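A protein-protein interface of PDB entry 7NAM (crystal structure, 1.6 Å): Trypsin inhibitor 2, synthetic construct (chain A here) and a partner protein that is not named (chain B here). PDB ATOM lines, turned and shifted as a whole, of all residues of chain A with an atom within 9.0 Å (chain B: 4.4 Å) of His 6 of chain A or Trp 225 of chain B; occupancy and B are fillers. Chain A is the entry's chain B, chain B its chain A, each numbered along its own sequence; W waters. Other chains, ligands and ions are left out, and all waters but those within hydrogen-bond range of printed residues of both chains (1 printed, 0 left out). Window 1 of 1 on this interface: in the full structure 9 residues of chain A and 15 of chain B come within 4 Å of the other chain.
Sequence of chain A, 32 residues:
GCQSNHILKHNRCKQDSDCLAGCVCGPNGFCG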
ATOM      1  N   CYS A   2       3.941  -0.564   9.331  1.00  0.00           N
ATOM      2  CA  CYS A   2       3.689   0.863   9.489  1.00  0.00           C
ATOM      3  C   CYS A   2       3.772   1.579   8.152  1.00  0.00           C
ATOM      4  O   CYS A   2       3.347   2.727   8.033  1.00  0.00           O
ATOM      5  CB  CYS A   2       4.682   1.486  10.470  1.00  0.00           C
ATOM      6  SG  CYS A   2       4.336   1.097  12.186  1.00  0.00           S
ATOM      7  N   GLN A   3       4.335   0.905   7.153  1.00  0.00           N
ATOM      8  CA  GLN A   3       4.452   1.492   5.826  1.00  0.00           C
ATOM      9  C   GLN A   3       3.083   1.494   5.174  1.00  0.00           C
ATOM     10  O   GLN A   3       2.508   0.453   4.880  1.00  0.00           O
ATOM     11  CB  GLN A   3       5.468   0.730   4.965  1.00  0.00           C
ATOM     12  CG  GLN A   3       5.712   1.342   3.573  1.00  0.00           C
ATOM     13  CD  GLN A   3       6.345   2.727   3.614  1.00  0.00           C
ATOM     14  OE1 GLN A   3       7.521   2.882   3.939  1.00  0.00           O
ATOM     15  NE2 GLN A   3       5.564   3.742   3.264  1.00  0.00           N
ATOM     16  N   SER A   4       2.546   2.684   4.974  1.00  0.00           N
ATOM     17  CA  SER A   4       1.282   2.823   4.279  1.00  0.00           C
ATOM     18  C   SER A   4       1.496   2.613   2.782  1.00  0.00           C
ATOM     19  O   SER A   4       2.584   2.878   2.278  1.00  0.00           O
ATOM     20  CB  SER A   4       0.698   4.207   4.553  1.00  0.00           C
ATOM     21  OG  SER A   4      -0.485   4.420   3.824  1.00  0.00           O
ATOM     22  N   ASN A   5       0.466   2.170   2.059  1.00  0.00           N
ATOM     23  CA  ASN A   5       0.569   2.167   0.596  1.00  0.00           C
ATOM     24  C   ASN A   5      -0.034   3.433  -0.020  1.00  0.00           C
ATOM     25  O   ASN A   5      -0.008   3.575  -1.232  1.00  0.00           O
ATOM     26  CB  ASN A   5      -0.099   0.921  -0.023  1.00  0.00           C
ATOM     27  CG  ASN A   5       0.446   0.597  -1.407  1.00  0.00           C
ATOM     28  OD1 ASN A   5       1.644   0.688  -1.640  1.00  0.00           O
ATOM     29  ND2 ASN A   5      -0.449   0.284  -2.342  1.00  0.00           N
ATOM     30  N   HIS A   6      -0.577   4.348   0.800  1.00  0.00           N
ATOM     31  CA  HIS A   6      -1.048   5.646   0.286  1.00  0.00           C
ATOM     32  C   HIS A   6       0.152   6.558   0.077  1.00  0.00           C
ATOM     33  O   HIS A   6       1.134   6.452   0.806  1.00  0.00           O
ATOM     34  CB  HIS A   6      -2.019   6.321   1.245  1.00  0.00           C
ATOM     35  CG  HIS A   6      -3.276   5.552   1.498  1.00  0.00           C
ATOM     36  ND1 HIS A   6      -4.382   5.631   0.677  1.00  0.00           N
ATOM     37  CD2 HIS A   6      -3.619   4.724   2.513  1.00  0.00           C
ATOM     38  CE1 HIS A   6      -5.344   4.865   1.163  1.00  0.00           C
ATOM     39  NE2 HIS A   6      -4.901   4.294   2.271  1.00  0.00           N
ATOM     40  N   ILE A   7       0.058   7.485  -0.880  1.00  0.00           N
ATOM     41  CA  ILE A   7       1.136   8.420  -1.125  1.00  0.00           C
ATOM     42  C   ILE A   7       1.234   9.446   0.001  1.00  0.00           C
ATOM     43  O   ILE A   7       2.342   9.807   0.397  1.00  0.00           O
ATOM     44  CB  ILE A   7       0.954   9.099  -2.490  1.00  0.00           C
ATOM     45  CG1 ILE A   7       1.212   8.043  -3.563  1.00  0.00           C
ATOM     46  CG2 ILE A   7       1.897  10.296  -2.662  1.00  0.00           C
ATOM     47  CD1 ILE A   7       0.841   8.472  -4.936  1.00  0.00           C
ATOM     48  N   LEU A   8       0.092   9.870   0.547  1.00  0.00           N
ATOM     49  CA  LEU A   8       0.069  10.858   1.633  1.00  0.00           C
ATOM     50  C   LEU A   8      -0.493  10.293   2.929  1.00  0.00           C
ATOM     51  O   LEU A   8       0.171  10.346   3.967  1.00  0.00           O
ATOM     52  CB  LEU A   8      -0.748  12.089   1.226  1.00  0.00           C
ATOM     53  CG  LEU A   8      -0.218  12.902   0.046  1.00  0.00           C
ATOM     54  CD1 LEU A   8      -1.125  14.119  -0.115  1.00  0.00           C
ATOM     55  CD2 LEU A   8       1.212  13.322   0.260  1.00  0.00           C
ATOM     56  N   LYS A   9      -1.707   9.752   2.877  1.00  0.00           N
ATOM     57  CA  LYS A   9      -2.400   9.313   4.084  1.00  0.00           C
ATOM     58  C   LYS A   9      -1.594   8.256   4.845  1.00  0.00           C
ATOM     59  O   LYS A   9      -1.193   7.259   4.274  1.00  0.00           O
ATOM     60  CB  LYS A   9      -3.783   8.759   3.724  1.00  0.00           C
ATOM     61  CG  LYS A   9      -4.645   8.376   4.921  1.00  0.00           C
ATOM     62  CD  LYS A   9      -5.701   7.336   4.558  1.00  0.00           C
ATOM     63  CE  LYS A   9      -7.046   7.961   4.232  1.00  0.00           C
ATOM     64  NZ  LYS A   9      -7.790   8.345   5.470  1.00  0.00           N
ATOM     65  N   HIS A  10      -1.359   8.496   6.135  1.00  0.00           N
ATOM     66  CA  HIS A  10      -0.606   7.563   7.001  1.00  0.00           C
ATOM     67  C   HIS A  10       0.824   7.347   6.515  1.00  0.00           C
ATOM     68  O   HIS A  10       1.464   6.363   6.885  1.00  0.00           O
ATOM     69  CB  HIS A  10      -1.308   6.199   7.090  1.00  0.00           C
ATOM     70  CG  HIS A  10      -2.721   6.270   7.569  1.00  0.00           C
ATOM     71  ND1 HIS A  10      -3.155   7.212   8.477  1.00  0.00           N
ATOM     72  CD2 HIS A  10      -3.802   5.515   7.262  1.00  0.00           C
ATOM     73  CE1 HIS A  10      -4.442   7.037   8.709  1.00  0.00           C
ATOM     74  NE2 HIS A  10      -4.859   6.012   7.987  1.00  0.00           N
ATOM     75  N   ASN A  11       1.308   8.255   5.671  1.00  0.00           N
ATOM     76  CA  ASN A  11       2.648   8.147   5.078  1.00  0.00           C
ATOM     77  C   ASN A  11       3.444   9.397   5.425  1.00  0.00           C
ATOM     78  O   ASN A  11       4.365   9.347   6.235  1.00  0.00           O
ATOM     79  CB  ASN A  11       2.567   7.941   3.558  1.00  0.00           C
ATOM     80  CG  ASN A  11       3.858   7.411   2.965  1.00  0.00           C
ATOM     81  OD1 ASN A  11       4.930   7.535   3.567  1.00  0.00           O
ATOM     82  ND2 ASN A  11       3.760   6.783   1.781  1.00  0.00           N
ATOM     83  N   ARG A  12       3.071  10.527   4.837  1.00  0.00           N
ATOM     84  CA  ARG A  12       3.537  11.816   5.327  1.00  0.00           C
ATOM     85  C   ARG A  12       2.977  12.031   6.726  1.00  0.00           C
ATOM     86  O   ARG A  12       1.861  11.572   7.014  1.00  0.00           O
ATOM     87  CB  ARG A  12       3.082  12.935   4.393  1.00  0.00           C
ATOM     88  CG  ARG A  12       3.911  13.080   3.145  1.00  0.00           C
ATOM     89  CD  ARG A  12       5.150  13.907   3.437  1.00  0.00           C
ATOM     90  NE  ARG A  12       5.781  14.396   2.218  1.00  0.00           N
ATOM     91  CZ  ARG A  12       6.950  15.017   2.179  1.00  0.00           C
ATOM     92  NH1 ARG A  12       7.443  15.410   1.010  1.00  0.00           N
ATOM     93  NH2 ARG A  12       7.632  15.239   3.299  1.00  0.00           N
ATOM     94  N   LEU A  20      -0.715   5.241  11.338  1.00  0.00           N
ATOM     95  CA  LEU A  20      -1.525   4.121  11.800  1.00  0.00           C
ATOM     96  C   LEU A  20      -1.245   3.865  13.276  1.00  0.00           C
ATOM     97  O   LEU A  20      -0.155   4.160  13.764  1.00  0.00           O
ATOM     98  CB  LEU A  20      -1.226   2.870  10.981  1.00  0.00           C
ATOM     99  CG  LEU A  20      -1.434   2.986   9.468  1.00  0.00           C
ATOM    100  CD1 LEU A  20      -0.614   1.945   8.721  1.00  0.00           C
ATOM    101  CD2 LEU A  20      -2.891   2.830   9.136  1.00  0.00           C
ATOM    102  N   ASN A  28      12.321  12.101   9.520  1.00  0.00           N
ATOM    103  CA  ASN A  28      12.276  12.555   8.135  1.00  0.00           C
ATOM    104  C   ASN A  28      10.875  13.020   7.733  1.00  0.00           C
ATOM    105  O   ASN A  28      10.665  13.461   6.607  1.00  0.00           O
ATOM    106  CB  ASN A  28      12.754  11.443   7.187  1.00  0.00           C
ATOM    107  CG  ASN A  28      11.913  10.176   7.287  1.00  0.00           C
ATOM    108  OD1 ASN A  28      11.177   9.980   8.256  1.00  0.00           O
ATOM    109  ND2 ASN A  28      12.028   9.303   6.284  1.00  0.00           N
ATOM    110  N   PHE A  30       8.076  10.992   7.907  1.00  0.00           N
ATOM    111  CA  PHE A  30       7.278   9.870   7.414  1.00  0.00           C
ATOM    112  C   PHE A  30       7.005   8.845   8.517  1.00  0.00           C
ATOM    113  O   PHE A  30       7.812   8.669   9.424  1.00  0.00           O
ATOM    114  CB  PHE A  30       7.985   9.197   6.235  1.00  0.00           C
ATOM    115  CG  PHE A  30       8.142  10.092   5.033  1.00  0.00           C
ATOM    116  CD1 PHE A  30       7.133  10.197   4.084  1.00  0.00           C
ATOM    117  CD2 PHE A  30       9.288  10.849   4.873  1.00  0.00           C
ATOM    118  CE1 PHE A  30       7.284  11.038   2.973  1.00  0.00           C
ATOM    119  CE2 PHE A  30       9.448  11.686   3.773  1.00  0.00           C
ATOM    120  CZ  PHE A  30       8.454  11.784   2.828  1.00  0.00           C
ATOM    121  N   CYS A  31       5.854   8.187   8.438  1.00  0.00           N
ATOM    122  CA  CYS A  31       5.461   7.179   9.417  1.00  0.00           C
ATOM    123  C   CYS A  31       6.339   5.942   9.306  1.00  0.00           C
ATOM    124  O   CYS A  31       6.755   5.575   8.208  1.00  0.00           O
ATOM    125  CB  CYS A  31       4.001   6.785   9.215  1.00  0.00           C
ATOM    126  SG  CYS A  31       2.832   8.152   9.399  1.00  0.00           S
ATOM    127  N   GLN B 122      -8.813   2.520  -5.771  1.00  0.00           N
ATOM    128  CA  GLN B 122      -7.462   3.066  -5.644  1.00  0.00           C
ATOM    129  C   GLN B 122      -6.675   2.834  -6.940  1.00  0.00           C
ATOM    130  O   GLN B 122      -5.681   2.102  -6.956  1.00  0.00           O
ATOM    131  CB  GLN B 122      -6.719   2.440  -4.459  1.00  0.00           C
ATOM    132  CG  GLN B 122      -7.337   2.736  -3.105  1.00  0.00           C
ATOM    133  CD  GLN B 122      -7.036   4.144  -2.592  1.00  0.00           C
ATOM    134  OE1 GLN B 122      -6.182   4.863  -3.126  1.00  0.00           O
ATOM    135  NE2 GLN B 122      -7.732   4.531  -1.532  1.00  0.00           N
ATOM    136  N   ARG B 124      -3.984   3.442  -9.765  1.00  0.00           N
ATOM    137  CA  ARG B 124      -2.602   3.831  -9.501  1.00  0.00           C
ATOM    138  C   ARG B 124      -1.824   3.857 -10.806  1.00  0.00           C
ATOM    139  O   ARG B 124      -1.844   4.874 -11.487  1.00  0.00           O
ATOM    140  CB  ARG B 124      -1.923   2.907  -8.471  1.00  0.00           C
ATOM    141  CG  ARG B 124      -0.476   3.305  -8.175  1.00  0.00           C
ATOM    142  CD  ARG B 124      -0.024   2.948  -6.794  1.00  0.00           C
ATOM    143  NE  ARG B 124      -0.501   3.905  -5.786  1.00  0.00           N
ATOM    144  CZ  ARG B 124      -0.232   3.841  -4.488  1.00  0.00           C
ATOM    145  NH1 ARG B 124       0.500   2.848  -3.953  1.00  0.00           N
ATOM    146  NH2 ARG B 124      -0.706   4.786  -3.690  1.00  0.00           N
ATOM    147  N   TRP B 140      -5.487  -0.880  -6.546  1.00  0.00           N
ATOM    148  CA  TRP B 140      -5.176  -1.616  -5.325  1.00  0.00           C
ATOM    149  C   TRP B 140      -6.223  -1.445  -4.232  1.00  0.00           C
ATOM    150  O   TRP B 140      -5.923  -1.587  -3.056  1.00  0.00           O
ATOM    151  CB  TRP B 140      -3.791  -1.205  -4.781  1.00  0.00           C
ATOM    152  CG  TRP B 140      -3.607   0.244  -4.388  1.00  0.00           C
ATOM    153  CD1 TRP B 140      -3.291   1.284  -5.222  1.00  0.00           C
ATOM    154  CD2 TRP B 140      -3.676   0.803  -3.065  1.00  0.00           C
ATOM    155  NE1 TRP B 140      -3.189   2.454  -4.504  1.00  0.00           N
ATOM    156  CE2 TRP B 140      -3.420   2.180  -3.178  1.00  0.00           C
ATOM    157  CE3 TRP B 140      -3.949   0.277  -1.803  1.00  0.00           C
ATOM    158  CZ2 TRP B 140      -3.417   3.030  -2.077  1.00  0.00           C
ATOM    159  CZ3 TRP B 140      -3.944   1.133  -0.704  1.00  0.00           C
ATOM    160  CH2 TRP B 140      -3.686   2.493  -0.855  1.00  0.00           C
ATOM    161  N   HIS B 209       8.519  -3.510  -0.534  1.00  0.00           N
ATOM    162  CA  HIS B 209       7.466  -2.547  -0.921  1.00  0.00           C
ATOM    163  C   HIS B 209       7.750  -1.841  -2.248  1.00  0.00           C
ATOM    164  O   HIS B 209       7.982  -0.617  -2.292  1.00  0.00           O
ATOM    165  CB  HIS B 209       7.250  -1.500   0.192  1.00  0.00           C
ATOM    166  CG  HIS B 209       5.904  -0.839   0.139  1.00  0.00           C
ATOM    167  ND1 HIS B 209       4.940  -1.032   1.107  1.00  0.00           N
ATOM    168  CD2 HIS B 209       5.355  -0.007  -0.775  1.00  0.00           C
ATOM    169  CE1 HIS B 209       3.856  -0.345   0.791  1.00  0.00           C
ATOM    170  NE2 HIS B 209       4.080   0.281  -0.349  1.00  0.00           N
ATOM    171  N   PHE B 211       7.180   0.239  -5.553  1.00  0.00           N
ATOM    172  CA  PHE B 211       6.181   1.219  -5.966  1.00  0.00           C
ATOM    173  C   PHE B 211       6.010   1.349  -7.473  1.00  0.00           C
ATOM    174  O   PHE B 211       4.868   1.461  -7.954  1.00  0.00           O
ATOM    175  CB  PHE B 211       6.504   2.595  -5.412  1.00  0.00           C
ATOM    176  CG  PHE B 211       5.501   3.647  -5.830  1.00  0.00           C
ATOM    177  CD1 PHE B 211       4.230   3.653  -5.273  1.00  0.00           C
ATOM    178  CD2 PHE B 211       5.823   4.597  -6.774  1.00  0.00           C
ATOM    179  CE1 PHE B 211       3.284   4.610  -5.653  1.00  0.00           C
ATOM    180  CE2 PHE B 211       4.894   5.571  -7.154  1.00  0.00           C
ATOM    181  CZ  PHE B 211       3.611   5.560  -6.591  1.00  0.00           C
ATOM    182  N   THR B 223      11.494   0.915  -8.138  1.00  0.00           N
ATOM    183  CA  THR B 223      11.701   1.638  -6.888  1.00  0.00           C
ATOM    184  C   THR B 223      11.034   0.877  -5.772  1.00  0.00           C
ATOM    185  O   THR B 223      10.021   0.208  -5.986  1.00  0.00           O
ATOM    186  CB  THR B 223      11.121   3.063  -6.938  1.00  0.00           C
ATOM    187  OG1 THR B 223       9.756   2.973  -7.330  1.00  0.00           O
ATOM    188  CG2 THR B 223      11.860   3.936  -7.927  1.00  0.00           C
ATOM    189  N   ASP B 224      11.616   0.966  -4.581  1.00  0.00           N
ATOM    190  CA  ASP B 224      11.041   0.317  -3.406  1.00  0.00           C
ATOM    191  C   ASP B 224      11.004   1.299  -2.242  1.00  0.00           C
ATOM    192  O   ASP B 224      12.009   1.895  -1.888  1.00  0.00           O
ATOM    193  CB  ASP B 224      11.844  -0.936  -3.034  1.00  0.00           C
ATOM    194  CG  ASP B 224      11.202  -1.728  -1.915  1.00  0.00           C
ATOM    195  OD1 ASP B 224      11.187  -1.225  -0.774  1.00  0.00           O
ATOM    196  OD2 ASP B 224      10.724  -2.860  -2.172  1.00  0.00           O
ATOM    197  N   TRP B 225       9.812   1.483  -1.680  1.00  0.00           N
ATOM    198  CA  TRP B 225       9.596   2.476  -0.630  1.00  0.00           C
ATOM    199  C   TRP B 225      10.266   2.160   0.691  1.00  0.00           C
ATOM    200  O   TRP B 225      10.604   3.071   1.451  1.00  0.00           O
ATOM    201  CB  TRP B 225       8.100   2.640  -0.386  1.00  0.00           C
ATOM    202  CG  TRP B 225       7.419   3.560  -1.343  1.00  0.00           C
ATOM    203  CD1 TRP B 225       7.947   4.142  -2.460  1.00  0.00           C
ATOM    204  CD2 TRP B 225       6.061   3.995  -1.263  1.00  0.00           C
ATOM    205  NE1 TRP B 225       6.992   4.918  -3.082  1.00  0.00           N
ATOM    206  CE2 TRP B 225       5.832   4.852  -2.363  1.00  0.00           C
ATOM    207  CE3 TRP B 225       5.015   3.748  -0.360  1.00  0.00           C
ATOM    208  CZ2 TRP B 225       4.598   5.459  -2.580  1.00  0.00           C
ATOM    209  CZ3 TRP B 225       3.801   4.347  -0.578  1.00  0.00           C
ATOM    210  CH2 TRP B 225       3.602   5.192  -1.680  1.00  0.00           C
ATOM    211  N   SER B 226      10.455   0.882   0.993  1.00  0.00           N
ATOM    212  CA  SER B 226      11.043   0.542   2.272  1.00  0.00           C
ATOM    213  C   SER B 226      12.574   0.478   2.172  1.00  0.00           C
ATOM    214  O   SER B 226      13.241   0.799   3.138  1.00  0.00           O
ATOM    215  CB  SER B 226      10.458  -0.765   2.797  1.00  0.00           C
ATOM    216  OG  SER B 226      10.834  -1.844   1.969  1.00  0.00           O
ATOM    217  N   THR B 227      13.131   0.112   1.011  1.00  0.00           N
ATOM    218  CA  THR B 227      14.592   0.088   0.834  1.00  0.00           C
ATOM    219  C   THR B 227      15.149   1.449   0.420  1.00  0.00           C
ATOM    220  O   THR B 227      16.359   1.658   0.443  1.00  0.00           O
ATOM    221  CB  THR B 227      15.049  -0.943  -0.233  1.00  0.00           C
ATOM    222  OG1 THR B 227      14.636  -0.528  -1.533  1.00  0.00           O
ATOM    223  CG2 THR B 227      14.500  -2.340   0.058  1.00  0.00           C
ATOM    224  N   HIS B 228      14.259   2.368   0.040  1.00  0.00           N
ATOM    225  CA  HIS B 228      14.660   3.691  -0.444  1.00  0.00           C
ATOM    226  C   HIS B 228      15.699   3.557  -1.539  1.00  0.00           C
ATOM    227  O   HIS B 228      16.735   4.228  -1.528  1.00  0.00           O
ATOM    228  CB  HIS B 228      15.208   4.555   0.696  1.00  0.00           C
ATOM    229  CG  HIS B 228      14.161   5.028   1.658  1.00  0.00           C
ATOM    230  ND1 HIS B 228      13.735   6.341   1.706  1.00  0.00           N
ATOM    231  CD2 HIS B 228      13.438   4.366   2.591  1.00  0.00           C
ATOM    232  CE1 HIS B 228      12.813   6.470   2.642  1.00  0.00           C
ATOM    233  NE2 HIS B 228      12.605   5.285   3.185  1.00  0.00           N
ATOM    234  N   PRO B 251      11.799   7.510  -3.108  1.00  0.00           N
ATOM    235  CA  PRO B 251      11.631   7.191  -4.529  1.00  0.00           C
ATOM    236  C   PRO B 251      10.190   6.885  -4.900  1.00  0.00           C
ATOM    237  O   PRO B 251       9.512   6.253  -4.097  1.00  0.00           O
ATOM    238  CB  PRO B 251      12.497   5.957  -4.708  1.00  0.00           C
ATOM    239  CG  PRO B 251      12.572   5.325  -3.321  1.00  0.00           C
ATOM    240  CD  PRO B 251      12.568   6.479  -2.378  1.00  0.00           C
ATOM    241  N   MET B 252       9.748   7.316  -6.076  1.00  0.00           N
ATOM    242  CA  MET B 252       8.363   7.164  -6.511  1.00  0.00           C
ATOM    243  C   MET B 252       8.333   6.544  -7.926  1.00  0.00           C
ATOM    244  O   MET B 252       8.899   5.463  -8.142  1.00  0.00           O
ATOM    245  CB  MET B 252       7.631   8.524  -6.453  1.00  0.00           C
ATOM    246  CG  MET B 252       7.711   9.188  -5.091  1.00  0.00           C
ATOM    247  SD  MET B 252       6.801   8.332  -3.771  1.00  0.00           S
ATOM    248  CE  MET B 252       5.138   8.921  -4.051  1.00  0.00           C
HETATM  249  O   HOH W   1      -2.257   7.280  -2.734  1.00  0.00           O
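The guanidinium group (NH2) of Arg 124 of chain B is in hydrogen-bond range of the backbone carbonyl oxygen (O) of Asn 5 of chain A (2.8 Å). A ring nitrogen (NE2) of His 209 of chain B is in hydrogen-bond range of the side-chain amide oxygen (OD1) of Asn 5 of chain A, at 2.8 Å.
The backbone carbonyl oxygen (O) of Gln 122 of chain B lies within hydrogen-bond range of the backbone NH (N) of Trp 140 of chain B. The backbone NH (N) of His 209 of chain B sits at hydrogen-bond distance from the side-chain carboxylate (OD2) of Asp 224 of chain B (2.8 Å). The side-chain hydroxyl (OG1) of Thr 223 of chain B lies within hydrogen-bond range of the backbone carbonyl oxygen (O) of Met 252 of chain B, at 2.8 Å. The backbone carbonyl oxygen (O) of Trp 225 of chain B lies close to a ring nitrogen (NE2) of His 228 of chain B. The indole nitrogen (NE1) of Trp 225 of chain B is in hydrogen-bond range of the side-chain sulfur (SD) of Met 252 of chain B. ND2 of Asn 11 of chain A lies within hydrogen-bond range of O of His 6 of chain A (2.8 Å).
Among the printed residues, merely in contact across the chains: Gln 3 of chain A with His 209 of chain B, Gln 3 of chain A with Trp 225 of chain B, Ser 4 of chain A with His 209 of chain B, Ser 4 of chain A with Trp 225 of chain B, Asn 5 of chain A with Trp 140 of chain B, Asn 5 of chain A with Trp 225 of chain B, His 6 of chain A with Gln 122 of chain B, His 6 of chain A with Trp 140 of chain B, His 6 of chain A with Trp 225 of chain B, Ile 7 of chain A with Arg 124 of chain B, Ile 7 of chain A with Met 252 of chain B and Asn 11 of chain A with Trp 225 of chain B.
Of chain B, only Gln 122 (3.6 Å), Trp 140 (3.5 Å) and Trp 225 (3.7 Å) come within 4 Å of His 6 of chain A. Trp 225 of chain B touches just these residues of chain A: Gln 3 (3.7 Å), Ser 4 (3.4 Å), Asn 5 (3.9 Å), His 6 (3.7 Å) and Asn 11 (3.4 Å). No residue of chain A comes within 4 Å of Asp 224 of chain B. No residue of chain A comes within 4 Å of Ser 226 of chain B. Of the printed residues of chain A, Met 252 of chain B touches Ile 7. Printed residues of chain A within 4 Å of Gln 122 of chain B: His 6 (3.6 Å). Printed residues of chain B within 4 Å of Ser 4 of chain A: His 209 and Trp 225. Printed residues of chain A within 4 Å of Trp 140 of chain B: Asn 5 (3.3 Å) and His 6 (3.5 Å). Printed residues of chain B within 4 Å of Gln 3 of chain A: His 209 (3.5 Å) and Trp 225 (3.7 Å). The nearest residue of chain A that does not touch Trp 225 of chain B is Ile 7 of chain A (4.1 Å). The nearest printed residue of chain A that does not touch Arg 124 of chain B is His 6 of chain A (4.1 Å).
Along chain A the printed residues that touch a printed residue of chain B span positions 3 to 11. Of the 13 printed residues of chain B, 6 touch a printed residue of chain A. Printed residues of chain B that touch a printed residue of chain A: Gln 122, Arg 124, Trp 140, His 209, Trp 225 and Met 252.
Water W1 lies within hydrogen-bond range of N of Ile 7 of chain A (3.0 Å) and NH2 of Arg 124 of chain B (3.1 Å).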
